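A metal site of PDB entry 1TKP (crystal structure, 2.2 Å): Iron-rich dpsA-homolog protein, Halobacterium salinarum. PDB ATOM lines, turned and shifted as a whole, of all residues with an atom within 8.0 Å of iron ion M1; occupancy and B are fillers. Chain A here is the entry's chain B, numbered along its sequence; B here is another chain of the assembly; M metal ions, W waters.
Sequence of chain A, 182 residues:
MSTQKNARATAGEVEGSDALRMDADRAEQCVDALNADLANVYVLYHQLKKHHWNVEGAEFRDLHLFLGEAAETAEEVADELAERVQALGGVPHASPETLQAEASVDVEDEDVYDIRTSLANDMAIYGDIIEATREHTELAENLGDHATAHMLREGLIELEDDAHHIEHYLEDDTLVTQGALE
The side-chain carboxylate of Asp 79 sits close to the indole nitrogen of Trp 53 of chain B (3.0 Å). The side-chain amino group of Lys 49 of chain B sits close to the side-chain carboxylate of Asp 79 (3.3 Å). The backbone NH (N) of Gly 68 of chain B is in hydrogen-bond range of a ring nitrogen (ND1) of His 52 of chain B (3.3 Å). O of His 64 of chain B is in hydrogen-bond range of ND1 of His 52 of chain B, 2.6 Å away.
Three residues have an atom within 4 Å of iron ion M1: Asp 79, Glu 83 and His 52 of chain B. Along chain A the residues within 4 Å of iron ion M1 span positions 79 to 83. The nearest printed residue that does not touch iron ion M1 is His 64 of chain B (4.3 Å).
OE1 of Glu 83 is bound to iron ion M1 (2.1 Å). Iron ion M1 is bound by water W2. Iron ion M1 is bound by water W1 (2.2 Å). The side-chain carboxylate (OD2) of Asp 79 is bound to iron ion M1, 2.2 Å away. NE2 of His 52 of chain B binds iron ion M1 (2.3 Å). Iron ion M1 is bound by OD1 of Asp 79, at 2.4 Å.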
ATOM      1  N   GLU A  75      22.347 -23.566  26.065  1.00  0.00           N
ATOM      2  CA  GLU A  75      23.001 -22.437  25.413  1.00  0.00           C
ATOM      3  C   GLU A  75      23.898 -22.852  24.247  1.00  0.00           C
ATOM      4  O   GLU A  75      23.981 -22.156  23.224  1.00  0.00           O
ATOM      5  CB  GLU A  75      23.839 -21.613  26.365  1.00  0.00           C
ATOM      6  CG  GLU A  75      24.283 -20.303  25.684  1.00  0.00           C
ATOM      7  CD  GLU A  75      25.328 -19.512  26.492  1.00  0.00           C
ATOM      8  OE1 GLU A  75      25.840 -20.050  27.571  1.00  0.00           O
ATOM      9  OE2 GLU A  75      25.639 -18.355  26.038  1.00  0.00           O
ATOM     10  N   GLU A  76      24.567 -23.971  24.453  1.00  0.00           N
ATOM     11  CA  GLU A  76      25.493 -24.507  23.511  1.00  0.00           C
ATOM     12  C   GLU A  76      24.710 -25.073  22.343  1.00  0.00           C
ATOM     13  O   GLU A  76      25.160 -24.929  21.195  1.00  0.00           O
ATOM     14  CB  GLU A  76      26.339 -25.612  24.100  1.00  0.00           C
ATOM     15  CG  GLU A  76      27.013 -25.083  25.329  1.00  0.00           C
ATOM     16  CD  GLU A  76      28.164 -25.931  25.825  1.00  0.00           C
ATOM     17  OE1 GLU A  76      28.506 -26.939  25.081  1.00  0.00           O
ATOM     18  OE2 GLU A  76      28.751 -25.543  26.910  1.00  0.00           O
ATOM     19  N   ALA A  78      21.750 -24.065  21.436  1.00  0.00           N
ATOM     20  CA  ALA A  78      21.326 -22.897  20.702  1.00  0.00           C
ATOM     21  C   ALA A  78      22.430 -22.401  19.801  1.00  0.00           C
ATOM     22  O   ALA A  78      22.236 -22.101  18.589  1.00  0.00           O
ATOM     23  CB  ALA A  78      20.942 -21.757  21.716  1.00  0.00           C
ATOM     24  N   ASP A  79      23.635 -22.283  20.383  1.00  0.00           N
ATOM     25  CA  ASP A  79      24.718 -21.787  19.584  1.00  0.00           C
ATOM     26  C   ASP A  79      24.942 -22.719  18.361  1.00  0.00           C
ATOM     27  O   ASP A  79      25.178 -22.273  17.325  1.00  0.00           O
ATOM     28  CB  ASP A  79      26.013 -21.719  20.425  1.00  0.00           C
ATOM     29  CG  ASP A  79      27.156 -21.098  19.665  1.00  0.00           C
ATOM     30  OD1 ASP A  79      27.101 -19.863  19.486  1.00  0.00           O
ATOM     31  OD2 ASP A  79      28.139 -21.732  19.188  1.00  0.00           O
ATOM     32  N   GLU A  80      24.958 -24.022  18.525  1.00  0.00           N
ATOM     33  CA  GLU A  80      25.193 -24.869  17.401  1.00  0.00           C
ATOM     34  C   GLU A  80      24.078 -24.706  16.316  1.00  0.00           C
ATOM     35  O   GLU A  80      24.396 -24.665  15.148  1.00  0.00           O
ATOM     36  CB  GLU A  80      25.344 -26.353  17.849  1.00  0.00           C
ATOM     37  CG  GLU A  80      26.761 -26.852  18.415  1.00  0.00           C
ATOM     38  CD  GLU A  80      28.017 -26.960  17.447  1.00  0.00           C
ATOM     39  OE1 GLU A  80      29.170 -26.511  17.887  1.00  0.00           O
ATOM     40  OE2 GLU A  80      27.983 -27.583  16.286  1.00  0.00           O
ATOM     41  N   ALA A  82      22.088 -21.948  15.804  1.00  0.00           N
ATOM     42  CA  ALA A  82      22.107 -20.683  15.134  1.00  0.00           C
ATOM     43  C   ALA A  82      23.244 -20.727  14.150  1.00  0.00           C
ATOM     44  O   ALA A  82      23.142 -20.251  13.023  1.00  0.00           O
ATOM     45  CB  ALA A  82      22.369 -19.554  16.070  1.00  0.00           C
ATOM     46  N   GLU A  83      24.351 -21.311  14.531  1.00  0.00           N
ATOM     47  CA  GLU A  83      25.460 -21.324  13.592  1.00  0.00           C
ATOM     48  C   GLU A  83      25.199 -22.163  12.369  1.00  0.00           C
ATOM     49  O   GLU A  83      25.682 -21.862  11.320  1.00  0.00           O
ATOM     50  CB  GLU A  83      26.734 -21.764  14.279  1.00  0.00           C
ATOM     51  CG  GLU A  83      27.218 -20.551  15.085  1.00  0.00           C
ATOM     52  CD  GLU A  83      28.341 -20.925  15.994  1.00  0.00           C
ATOM     53  OE1 GLU A  83      28.879 -20.028  16.680  1.00  0.00           O
ATOM     54  OE2 GLU A  83      28.640 -22.149  16.014  1.00  0.00           O
ATOM     55  N   LYS B  49      26.029 -12.356  20.557  1.00  0.00           N
ATOM     56  CA  LYS B  49      25.823 -13.669  19.915  1.00  0.00           C
ATOM     57  C   LYS B  49      25.451 -13.488  18.441  1.00  0.00           C
ATOM     58  O   LYS B  49      25.995 -14.107  17.517  1.00  0.00           O
ATOM     59  CB  LYS B  49      24.705 -14.432  20.615  1.00  0.00           C
ATOM     60  CG  LYS B  49      24.999 -14.983  21.967  1.00  0.00           C
ATOM     61  CD  LYS B  49      26.226 -15.806  22.053  1.00  0.00           C
ATOM     62  CE  LYS B  49      26.131 -17.103  21.470  1.00  0.00           C
ATOM     63  NZ  LYS B  49      27.096 -18.133  22.250  1.00  0.00           N
ATOM     64  N   HIS B  52      28.469 -12.546  16.514  1.00  0.00           N
ATOM     65  CA  HIS B  52      29.326 -13.687  16.483  1.00  0.00           C
ATOM     66  C   HIS B  52      28.898 -14.718  15.454  1.00  0.00           C
ATOM     67  O   HIS B  52      29.743 -15.130  14.641  1.00  0.00           O
ATOM     68  CB  HIS B  52      29.256 -14.234  17.945  1.00  0.00           C
ATOM     69  CG  HIS B  52      29.737 -15.631  18.145  1.00  0.00           C
ATOM     70  ND1 HIS B  52      31.077 -15.950  18.318  1.00  0.00           N
ATOM     71  CD2 HIS B  52      29.043 -16.756  18.429  1.00  0.00           C
ATOM     72  CE1 HIS B  52      31.183 -17.242  18.615  1.00  0.00           C
ATOM     73  NE2 HIS B  52      29.953 -17.744  18.727  1.00  0.00           N
ATOM     74  N   TRP B  53      27.635 -15.174  15.529  1.00  0.00           N
ATOM     75  CA  TRP B  53      27.025 -15.955  14.448  1.00  0.00           C
ATOM     76  C   TRP B  53      27.251 -15.402  13.083  1.00  0.00           C
ATOM     77  O   TRP B  53      27.660 -16.142  12.214  1.00  0.00           O
ATOM     78  CB  TRP B  53      25.517 -16.079  14.559  1.00  0.00           C
ATOM     79  CG  TRP B  53      25.198 -16.763  15.909  1.00  0.00           C
ATOM     80  CD1 TRP B  53      26.017 -17.603  16.649  1.00  0.00           C
ATOM     81  CD2 TRP B  53      24.018 -16.633  16.626  1.00  0.00           C
ATOM     82  NE1 TRP B  53      25.383 -18.013  17.795  1.00  0.00           N
ATOM     83  CE2 TRP B  53      24.133 -17.439  17.794  1.00  0.00           C
ATOM     84  CE3 TRP B  53      22.818 -15.957  16.388  1.00  0.00           C
ATOM     85  CZ2 TRP B  53      23.118 -17.535  18.724  1.00  0.00           C
ATOM     86  CZ3 TRP B  53      21.824 -16.050  17.295  1.00  0.00           C
ATOM     87  CH2 TRP B  53      21.979 -16.822  18.462  1.00  0.00           C
ATOM     88  N   HIS B  64      34.829 -13.388  15.463  1.00  0.00           N
ATOM     89  CA  HIS B  64      33.894 -14.446  15.798  1.00  0.00           C
ATOM     90  C   HIS B  64      34.350 -14.917  17.167  1.00  0.00           C
ATOM     91  O   HIS B  64      33.583 -15.133  18.099  1.00  0.00           O
ATOM     92  CB  HIS B  64      33.976 -15.587  14.748  1.00  0.00           C
ATOM     93  CG  HIS B  64      33.185 -16.783  15.114  1.00  0.00           C
ATOM     94  ND1 HIS B  64      31.831 -16.876  14.883  1.00  0.00           N
ATOM     95  CD2 HIS B  64      33.546 -17.960  15.685  1.00  0.00           C
ATOM     96  CE1 HIS B  64      31.359 -18.001  15.400  1.00  0.00           C
ATOM     97  NE2 HIS B  64      32.389 -18.690  15.875  1.00  0.00           N
ATOM     98  N   LEU B  65      35.646 -14.961  17.346  1.00  0.00           N
ATOM     99  CA  LEU B  65      36.045 -15.415  18.627  1.00  0.00           C
ATOM    100  C   LEU B  65      35.934 -14.274  19.612  1.00  0.00           C
ATOM    101  O   LEU B  65      35.561 -14.505  20.725  1.00  0.00           O
ATOM    102  CB  LEU B  65      37.454 -15.872  18.565  1.00  0.00           C
ATOM    103  CG  LEU B  65      37.661 -17.098  17.695  1.00  0.00           C
ATOM    104  CD1 LEU B  65      39.202 -17.377  17.488  1.00  0.00           C
ATOM    105  CD2 LEU B  65      36.841 -18.289  18.261  1.00  0.00           C
ATOM    106  N   LEU B  67      33.746 -11.922  19.695  1.00  0.00           N
ATOM    107  CA  LEU B  67      32.396 -11.562  19.996  1.00  0.00           C
ATOM    108  C   LEU B  67      31.813 -12.701  20.814  1.00  0.00           C
ATOM    109  O   LEU B  67      30.978 -12.486  21.708  1.00  0.00           O
ATOM    110  CB  LEU B  67      31.673 -11.291  18.665  1.00  0.00           C
ATOM    111  CG  LEU B  67      32.013 -10.031  17.902  1.00  0.00           C
ATOM    112  CD1 LEU B  67      31.271 -10.138  16.594  1.00  0.00           C
ATOM    113  CD2 LEU B  67      31.358  -8.865  18.630  1.00  0.00           C
ATOM    114  N   GLY B  68      32.321 -13.930  20.657  1.00  0.00           N
ATOM    115  CA  GLY B  68      31.805 -15.045  21.482  1.00  0.00           C
ATOM    116  C   GLY B  68      32.310 -14.931  22.918  1.00  0.00           C
ATOM    117  O   GLY B  68      31.590 -15.147  23.877  1.00  0.00           O
HETATM  118 FE    FE M   1      29.352 -19.930  18.724  1.00  0.00          FE
HETATM  119 FE    FE M   2      28.236 -19.865  11.485  1.00  0.00          FE
HETATM  120  O   HOH W   1      31.393 -20.594  18.298  1.00  0.00           O
HETATM  121  O   HOH W   2      29.733 -19.848  20.846  1.00  0.00           O
